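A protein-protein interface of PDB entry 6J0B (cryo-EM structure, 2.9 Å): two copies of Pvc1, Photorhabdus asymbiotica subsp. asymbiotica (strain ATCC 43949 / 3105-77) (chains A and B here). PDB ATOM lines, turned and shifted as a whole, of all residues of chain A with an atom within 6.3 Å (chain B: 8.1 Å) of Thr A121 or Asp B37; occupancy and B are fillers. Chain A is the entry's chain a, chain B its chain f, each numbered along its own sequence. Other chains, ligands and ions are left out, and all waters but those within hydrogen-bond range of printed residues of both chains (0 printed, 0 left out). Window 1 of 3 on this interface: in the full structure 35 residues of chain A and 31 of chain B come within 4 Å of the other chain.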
ATOM      1  N   SER A 119     -23.279  29.341  28.973  1.00  0.00           N
ATOM      2  CA  SER A 119     -23.902  29.503  27.655  1.00  0.00           C
ATOM      3  C   SER A 119     -22.906  29.499  26.487  1.00  0.00           C
ATOM      4  O   SER A 119     -22.723  30.500  25.799  1.00  0.00           O
ATOM      5  CB  SER A 119     -24.767  30.768  27.620  1.00  0.00           C
ATOM      6  OG  SER A 119     -25.388  30.918  26.356  1.00  0.00           O
ATOM      7  N   LEU A 120     -22.262  28.357  26.270  1.00  0.00           N
ATOM      8  CA  LEU A 120     -21.514  28.164  25.033  1.00  0.00           C
ATOM      9  C   LEU A 120     -22.478  27.928  23.883  1.00  0.00           C
ATOM     10  O   LEU A 120     -23.334  27.046  23.957  1.00  0.00           O
ATOM     11  CB  LEU A 120     -20.556  26.984  25.152  1.00  0.00           C
ATOM     12  CG  LEU A 120     -19.804  26.616  23.876  1.00  0.00           C
ATOM     13  CD1 LEU A 120     -18.842  27.713  23.490  1.00  0.00           C
ATOM     14  CD2 LEU A 120     -19.073  25.314  24.055  1.00  0.00           C
ATOM     15  N   THR A 121     -22.334  28.703  22.815  1.00  0.00           N
ATOM     16  CA  THR A 121     -23.250  28.664  21.683  1.00  0.00           C
ATOM     17  C   THR A 121     -22.602  27.927  20.520  1.00  0.00           C
ATOM     18  O   THR A 121     -21.529  28.318  20.054  1.00  0.00           O
ATOM     19  CB  THR A 121     -23.660  30.073  21.264  1.00  0.00           C
ATOM     20  OG1 THR A 121     -24.348  30.707  22.346  1.00  0.00           O
ATOM     21  CG2 THR A 121     -24.577  30.023  20.067  1.00  0.00           C
ATOM     22  N   SER A 122     -23.255  26.873  20.058  1.00  0.00           N
ATOM     23  CA  SER A 122     -22.814  26.054  18.942  1.00  0.00           C
ATOM     24  C   SER A 122     -23.091  26.772  17.623  1.00  0.00           C
ATOM     25  O   SER A 122     -23.972  27.632  17.559  1.00  0.00           O
ATOM     26  CB  SER A 122     -23.547  24.720  18.966  1.00  0.00           C
ATOM     27  OG  SER A 122     -22.853  23.693  18.290  1.00  0.00           O
ATOM     28  N   PRO A 123     -22.340  26.457  16.563  1.00  0.00           N
ATOM     29  CA  PRO A 123     -22.609  27.081  15.266  1.00  0.00           C
ATOM     30  C   PRO A 123     -23.943  26.659  14.680  1.00  0.00           C
ATOM     31  O   PRO A 123     -24.469  25.582  14.968  1.00  0.00           O
ATOM     32  CB  PRO A 123     -21.452  26.589  14.392  1.00  0.00           C
ATOM     33  CG  PRO A 123     -20.937  25.387  15.085  1.00  0.00           C
ATOM     34  CD  PRO A 123     -21.070  25.714  16.526  1.00  0.00           C
ATOM     35  N   VAL A 134     -18.695  29.479  13.791  1.00  0.00           N
ATOM     36  CA  VAL A 134     -18.256  30.313  14.903  1.00  0.00           C
ATOM     37  C   VAL A 134     -18.987  29.885  16.165  1.00  0.00           C
ATOM     38  O   VAL A 134     -20.074  29.304  16.112  1.00  0.00           O
ATOM     39  CB  VAL A 134     -18.482  31.815  14.634  1.00  0.00           C
ATOM     40  CG1 VAL A 134     -17.260  32.426  13.989  1.00  0.00           C
ATOM     41  CG2 VAL A 134     -19.693  32.015  13.758  1.00  0.00           C
ATOM     42  N   GLN A 135     -18.376  30.181  17.306  1.00  0.00           N
ATOM     43  CA  GLN A 135     -18.941  29.899  18.615  1.00  0.00           C
ATOM     44  C   GLN A 135     -18.815  31.122  19.501  1.00  0.00           C
ATOM     45  O   GLN A 135     -17.755  31.747  19.552  1.00  0.00           O
ATOM     46  CB  GLN A 135     -18.225  28.753  19.301  1.00  0.00           C
ATOM     47  CG  GLN A 135     -18.461  27.399  18.726  1.00  0.00           C
ATOM     48  CD  GLN A 135     -17.636  26.361  19.437  1.00  0.00           C
ATOM     49  OE1 GLN A 135     -16.468  26.591  19.745  1.00  0.00           O
ATOM     50  NE2 GLN A 135     -18.242  25.216  19.723  1.00  0.00           N
ATOM     51  N   GLU A 136     -19.883  31.448  20.217  1.00  0.00           N
ATOM     52  CA  GLU A 136     -19.811  32.418  21.295  1.00  0.00           C
ATOM     53  C   GLU A 136     -19.794  31.693  22.627  1.00  0.00           C
ATOM     54  O   GLU A 136     -20.603  30.795  22.865  1.00  0.00           O
ATOM     55  CB  GLU A 136     -20.994  33.381  21.269  1.00  0.00           C
ATOM     56  CG  GLU A 136     -20.905  34.464  20.233  1.00  0.00           C
ATOM     57  CD  GLU A 136     -22.270  34.963  19.827  1.00  0.00           C
ATOM     58  OE1 GLU A 136     -22.513  36.185  19.898  1.00  0.00           O
ATOM     59  OE2 GLU A 136     -23.109  34.121  19.442  1.00  0.00           O
ATOM     60  N   ILE A 137     -18.870  32.083  23.492  1.00  0.00           N
ATOM     61  CA  ILE A 137     -18.910  31.709  24.895  1.00  0.00           C
ATOM     62  C   ILE A 137     -19.234  32.971  25.679  1.00  0.00           C
ATOM     63  O   ILE A 137     -18.856  34.077  25.280  1.00  0.00           O
ATOM     64  CB  ILE A 137     -17.597  31.032  25.350  1.00  0.00           C
ATOM     65  CG1 ILE A 137     -17.772  30.336  26.699  1.00  0.00           C
ATOM     66  CG2 ILE A 137     -16.426  31.991  25.390  1.00  0.00           C
ATOM     67  CD1 ILE A 137     -16.650  29.403  27.029  1.00  0.00           C
ATOM     68  N   THR A 138     -20.014  32.821  26.738  1.00  0.00           N
ATOM     69  CA  THR A 138     -20.408  33.937  27.580  1.00  0.00           C
ATOM     70  C   THR A 138     -19.756  33.753  28.942  1.00  0.00           C
ATOM     71  O   THR A 138     -19.692  32.639  29.460  1.00  0.00           O
ATOM     72  CB  THR A 138     -21.933  34.021  27.683  1.00  0.00           C
ATOM     73  OG1 THR A 138     -22.488  34.138  26.370  1.00  0.00           O
ATOM     74  CG2 THR A 138     -22.369  35.205  28.495  1.00  0.00           C
ATOM     75  N   SER B  34     -30.217  24.396  13.932  1.00  0.00           N
ATOM     76  CA  SER B  34     -30.114  25.596  14.750  1.00  0.00           C
ATOM     77  C   SER B  34     -30.228  25.248  16.228  1.00  0.00           C
ATOM     78  O   SER B  34     -30.573  24.129  16.603  1.00  0.00           O
ATOM     79  CB  SER B  34     -31.188  26.617  14.371  1.00  0.00           C
ATOM     80  OG  SER B  34     -31.236  27.665  15.318  1.00  0.00           O
ATOM     81  N   GLY B  35     -29.943  26.235  17.070  1.00  0.00           N
ATOM     82  CA  GLY B  35     -29.995  26.009  18.509  1.00  0.00           C
ATOM     83  C   GLY B  35     -28.741  25.309  18.982  1.00  0.00           C
ATOM     84  O   GLY B  35     -27.620  25.744  18.688  1.00  0.00           O
ATOM     85  N   LEU B  36     -28.936  24.249  19.769  1.00  0.00           N
ATOM     86  CA  LEU B  36     -27.921  23.240  20.084  1.00  0.00           C
ATOM     87  C   LEU B  36     -26.784  23.809  20.940  1.00  0.00           C
ATOM     88  O   LEU B  36     -25.621  23.451  20.795  1.00  0.00           O
ATOM     89  CB  LEU B  36     -27.386  22.600  18.794  1.00  0.00           C
ATOM     90  CG  LEU B  36     -26.724  21.231  18.788  1.00  0.00           C
ATOM     91  CD1 LEU B  36     -27.662  20.319  19.433  1.00  0.00           C
ATOM     92  CD2 LEU B  36     -26.464  20.794  17.390  1.00  0.00           C
ATOM     93  N   ASP B  37     -27.132  24.675  21.881  1.00  0.00           N
ATOM     94  CA  ASP B  37     -26.108  25.315  22.691  1.00  0.00           C
ATOM     95  C   ASP B  37     -26.275  24.976  24.165  1.00  0.00           C
ATOM     96  O   ASP B  37     -27.386  24.744  24.643  1.00  0.00           O
ATOM     97  CB  ASP B  37     -26.122  26.826  22.504  1.00  0.00           C
ATOM     98  CG  ASP B  37     -27.400  27.465  22.967  1.00  0.00           C
ATOM     99  OD1 ASP B  37     -28.314  27.630  22.137  1.00  0.00           O
ATOM    100  OD2 ASP B  37     -27.493  27.814  24.159  1.00  0.00           O
ATOM    101  N   ILE B  38     -25.150  24.957  24.877  1.00  0.00           N
ATOM    102  CA  ILE B  38     -25.129  24.803  26.327  1.00  0.00           C
ATOM    103  C   ILE B  38     -25.529  26.129  26.962  1.00  0.00           C
ATOM    104  O   ILE B  38     -25.420  27.178  26.329  1.00  0.00           O
ATOM    105  CB  ILE B  38     -23.728  24.343  26.775  1.00  0.00           C
ATOM    106  CG1 ILE B  38     -23.231  23.252  25.836  1.00  0.00           C
ATOM    107  CG2 ILE B  38     -23.734  23.795  28.182  1.00  0.00           C
ATOM    108  CD1 ILE B  38     -21.896  22.693  26.212  1.00  0.00           C
ATOM    109  N   SER B  39     -26.058  26.084  28.187  1.00  0.00           N
ATOM    110  CA  SER B  39     -26.372  27.283  28.953  1.00  0.00           C
ATOM    111  C   SER B  39     -26.448  26.926  30.427  1.00  0.00           C
ATOM    112  O   SER B  39     -26.713  25.781  30.792  1.00  0.00           O
ATOM    113  CB  SER B  39     -27.684  27.928  28.503  1.00  0.00           C
ATOM    114  OG  SER B  39     -27.814  29.224  29.057  1.00  0.00           O
ATOM    115  N   TYR B  40     -26.202  27.921  31.278  1.00  0.00           N
ATOM    116  CA  TYR B  40     -26.249  27.721  32.719  1.00  0.00           C
ATOM    117  C   TYR B  40     -26.837  28.950  33.386  1.00  0.00           C
ATOM    118  O   TYR B  40     -26.483  30.078  33.035  1.00  0.00           O
ATOM    119  CB  TYR B  40     -24.857  27.446  33.295  1.00  0.00           C
ATOM    120  CG  TYR B  40     -24.361  26.044  33.073  1.00  0.00           C
ATOM    121  CD1 TYR B  40     -23.700  25.703  31.909  1.00  0.00           C
ATOM    122  CD2 TYR B  40     -24.540  25.065  34.035  1.00  0.00           C
ATOM    123  CE1 TYR B  40     -23.251  24.428  31.695  1.00  0.00           C
ATOM    124  CE2 TYR B  40     -24.087  23.781  33.831  1.00  0.00           C
ATOM    125  CZ  TYR B  40     -23.444  23.472  32.656  1.00  0.00           C
ATOM    126  OH  TYR B  40     -22.984  22.198  32.432  1.00  0.00           O
ATOM    127  N   SER B  59     -28.491  23.746  35.077  1.00  0.00           N
ATOM    128  CA  SER B  59     -28.388  23.717  33.627  1.00  0.00           C
ATOM    129  C   SER B  59     -29.745  23.973  32.984  1.00  0.00           C
ATOM    130  O   SER B  59     -30.796  23.768  33.594  1.00  0.00           O
ATOM    131  CB  SER B  59     -27.841  22.370  33.170  1.00  0.00           C
ATOM    132  OG  SER B  59     -27.923  22.245  31.766  1.00  0.00           O
ATOM    133  N   GLN B  60     -29.718  24.435  31.740  1.00  0.00           N
ATOM    134  CA  GLN B  60     -30.934  24.722  30.996  1.00  0.00           C
ATOM    135  C   GLN B  60     -31.202  23.630  29.969  1.00  0.00           C
ATOM    136  O   GLN B  60     -30.286  22.943  29.513  1.00  0.00           O
ATOM    137  CB  GLN B  60     -30.846  26.073  30.294  1.00  0.00           C
ATOM    138  CG  GLN B  60     -30.848  27.257  31.226  1.00  0.00           C
ATOM    139  CD  GLN B  60     -31.299  28.524  30.535  1.00  0.00           C
ATOM    140  OE1 GLN B  60     -30.762  29.601  30.778  1.00  0.00           O
ATOM    141  NE2 GLN B  60     -32.301  28.400  29.671  1.00  0.00           N
ATOM    142  N   SER B  61     -32.474  23.484  29.604  1.00  0.00           N
ATOM    143  CA  SER B  61     -32.865  22.442  28.665  1.00  0.00           C
ATOM    144  C   SER B  61     -32.487  22.834  27.247  1.00  0.00           C
ATOM    145  O   SER B  61     -32.619  23.993  26.848  1.00  0.00           O
ATOM    146  CB  SER B  61     -34.365  22.176  28.746  1.00  0.00           C
ATOM    147  OG  SER B  61     -34.687  20.929  28.153  1.00  0.00           O
ATOM    148  N   THR B  62     -32.026  21.853  26.484  1.00  0.00           N
ATOM    149  CA  THR B  62     -31.536  22.083  25.136  1.00  0.00           C
ATOM    150  C   THR B  62     -32.677  21.984  24.133  1.00  0.00           C
ATOM    151  O   THR B  62     -33.408  20.992  24.114  1.00  0.00           O
ATOM    152  CB  THR B  62     -30.449  21.072  24.789  1.00  0.00           C
ATOM    153  OG1 THR B  62     -29.339  21.235  25.680  1.00  0.00           O
ATOM    154  CG2 THR B  62     -29.998  21.287  23.377  1.00  0.00           C
ATOM    155  N   ASN B  63     -32.813  23.006  23.291  1.00  0.00           N
ATOM    156  CA  ASN B  63     -33.859  23.063  22.282  1.00  0.00           C
ATOM    157  C   ASN B  63     -33.225  23.263  20.912  1.00  0.00           C
ATOM    158  O   ASN B  63     -32.554  24.272  20.681  1.00  0.00           O
ATOM    159  CB  ASN B  63     -34.846  24.183  22.604  1.00  0.00           C
ATOM    160  CG  ASN B  63     -36.094  24.108  21.771  1.00  0.00           C
ATOM    161  OD1 ASN B  63     -36.145  24.650  20.672  1.00  0.00           O
ATOM    162  ND2 ASN B  63     -37.118  23.438  22.289  1.00  0.00           N
ATOM    163  N   ILE B  64     -33.445  22.306  20.009  1.00  0.00           N
ATOM    164  CA  ILE B  64     -32.817  22.250  18.692  1.00  0.00           C
ATOM    165  C   ILE B  64     -33.899  22.407  17.635  1.00  0.00           C
ATOM    166  O   ILE B  64     -35.023  21.933  17.822  1.00  0.00           O
ATOM    167  CB  ILE B  64     -32.068  20.914  18.496  1.00  0.00           C
ATOM    168  CG1 ILE B  64     -31.314  20.535  19.762  1.00  0.00           C
ATOM    169  CG2 ILE B  64     -31.106  20.961  17.327  1.00  0.00           C
ATOM    170  CD1 ILE B  64     -31.886  19.334  20.457  1.00  0.00           C
ATOM    171  N   TRP B 110     -21.048  16.915  17.065  1.00  0.00           N
ATOM    172  CA  TRP B 110     -21.915  17.222  18.189  1.00  0.00           C
ATOM    173  C   TRP B 110     -22.839  16.040  18.432  1.00  0.00           C
ATOM    174  O   TRP B 110     -23.245  15.357  17.494  1.00  0.00           O
ATOM    175  CB  TRP B 110     -22.735  18.486  17.925  1.00  0.00           C
ATOM    176  CG  TRP B 110     -21.937  19.741  18.011  1.00  0.00           C
ATOM    177  CD1 TRP B 110     -21.894  20.605  19.057  1.00  0.00           C
ATOM    178  CD2 TRP B 110     -21.060  20.274  17.015  1.00  0.00           C
ATOM    179  NE1 TRP B 110     -21.048  21.645  18.778  1.00  0.00           N
ATOM    180  CE2 TRP B 110     -20.522  21.465  17.528  1.00  0.00           C
ATOM    181  CE3 TRP B 110     -20.681  19.862  15.735  1.00  0.00           C
ATOM    182  CZ2 TRP B 110     -19.625  22.244  16.812  1.00  0.00           C
ATOM    183  CZ3 TRP B 110     -19.793  20.637  15.029  1.00  0.00           C
ATOM    184  CH2 TRP B 110     -19.271  21.812  15.568  1.00  0.00           C
ATOM    185  N   VAL B 112     -26.354  14.802  20.636  1.00  0.00           N
ATOM    186  CA  VAL B 112     -27.526  15.175  21.415  1.00  0.00           C
ATOM    187  C   VAL B 112     -28.171  13.900  21.929  1.00  0.00           C
ATOM    188  O   VAL B 112     -28.322  12.932  21.179  1.00  0.00           O
ATOM    189  CB  VAL B 112     -28.533  15.987  20.586  1.00  0.00           C
ATOM    190  CG1 VAL B 112     -29.233  16.946  21.461  1.00  0.00           C
ATOM    191  CG2 VAL B 112     -27.846  16.733  19.491  1.00  0.00           C
ATOM    192  N   ARG B 143     -27.949  17.353  27.159  1.00  0.00           N
ATOM    193  CA  ARG B 143     -26.552  16.953  26.972  1.00  0.00           C
ATOM    194  C   ARG B 143     -26.117  17.056  25.505  1.00  0.00           C
ATOM    195  O   ARG B 143     -26.068  16.079  24.756  1.00  0.00           O
ATOM    196  CB  ARG B 143     -26.269  15.558  27.540  1.00  0.00           C
ATOM    197  CG  ARG B 143     -24.785  15.227  27.508  1.00  0.00           C
ATOM    198  CD  ARG B 143     -24.282  14.729  28.799  1.00  0.00           C
ATOM    199  NE  ARG B 143     -22.834  14.557  28.819  1.00  0.00           N
ATOM    200  CZ  ARG B 143     -22.181  13.521  28.300  1.00  0.00           C
ATOM    201  NH1 ARG B 143     -20.861  13.474  28.388  1.00  0.00           N
ATOM    202  NH2 ARG B 143     -22.832  12.541  27.686  1.00  0.00           N
ATOM    203  N   VAL B 144     -25.920  18.292  25.077  1.00  0.00           N
ATOM    204  CA  VAL B 144     -25.065  18.537  23.923  1.00  0.00           C
ATOM    205  C   VAL B 144     -23.621  18.388  24.364  1.00  0.00           C
ATOM    206  O   VAL B 144     -23.177  19.062  25.298  1.00  0.00           O
ATOM    207  CB  VAL B 144     -25.310  19.923  23.331  1.00  0.00           C
ATOM    208  CG1 VAL B 144     -24.389  20.161  22.158  1.00  0.00           C
ATOM    209  CG2 VAL B 144     -26.687  19.995  22.899  1.00  0.00           C
ATOM    210  N   MET B 146     -19.628  18.146  22.454  1.00  0.00           N
ATOM    211  CA  MET B 146     -18.888  18.399  21.229  1.00  0.00           C
ATOM    212  C   MET B 146     -17.639  17.533  21.235  1.00  0.00           C
ATOM    213  O   MET B 146     -16.854  17.580  22.185  1.00  0.00           O
ATOM    214  CB  MET B 146     -18.532  19.882  21.127  1.00  0.00           C
ATOM    215  CG  MET B 146     -17.520  20.260  20.077  1.00  0.00           C
ATOM    216  SD  MET B 146     -17.213  22.031  20.216  1.00  0.00           S
ATOM    217  CE  MET B 146     -16.280  22.369  18.737  1.00  0.00           C
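Among the printed residues, pairs that only touch across the chains: Ser A119 with Ile B38 (3.1 Å), Ser A119 with Ser B39 (3.6 Å), Ser A119 with Tyr B40 (3.98 Å), Leu A120 with Asp B37 (3.2 Å), Thr A121 with Asp B37 (3.5 Å), Ser A122 with Leu B36 (3.0 Å), Ser A122 with Asp B37 (3.8 Å) and Pro A123 with Trp B110 (3.8 Å).
No position is printed for both chains. Of the 11 pairs that touch across the chains among the printed residues, none has its exchanged pair printed and touching as well.
The backbone carbonyl oxygen of Glu A136 sits at hydrogen-bond distance from the backbone NH of Thr A121 (2.7 Å). The backbone NH (N) of Gln B60 is in hydrogen-bond range of the backbone carbonyl oxygen (O) of Ser B39.
The backbone NH (N) of Ile B38 sits at hydrogen-bond distance from the backbone carbonyl oxygen (O) of Leu A120 (2.9 Å). OG of Ser A122 lies within hydrogen-bond range of NE1 of Trp B110, at 2.8 Å. The side-chain amide nitrogen (NE2) of Gln A135 is in hydrogen-bond range of the side-chain sulfur (SD) of Met B146, 3.4 Å away.
Of the 18 printed residues of chain B, 7 touch a printed residue of chain A. Hydrophobic or aromatic side chains of chain B within 4 Å of the printed part of chain A: Ile B38, Trp B110 and Met B146. Of the 10 printed residues of chain A, 6 touch a printed residue of chain B. Printed residues of chain A that touch a printed residue of chain B: Ser A119, Leu A120, Thr A121, Ser A122, Pro A123 and Gln A135. Among the printed residues, no Asp or Glu carboxylate lies within 4 Å of a Lys or Arg side-chain nitrogen of the other chain.
Of chain B, only Asp B37 comes within 4 Å of Thr A121. Asp B37 touches three residues of chain A. Of the printed residues of chain A, Tyr B40 touches Ser A119 (3.98 Å). Of the printed residues of chain A, Met B146 touches Gln A135. Of the printed residues of chain A, Trp B110 touches Ser A122 and Pro A123. Printed residues of chain A within 4 Å of Leu B36: Ser A122. Thr B62 touches none of the printed residues of chain A. Ser B34 touches none of the printed residues of chain A. The nearest residue of chain A that does not touch Asp B37 is Ser A119 (4.3 Å). The nearest printed residue of chain A that does not touch Leu B36 is Leu A120 (5.3 Å).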
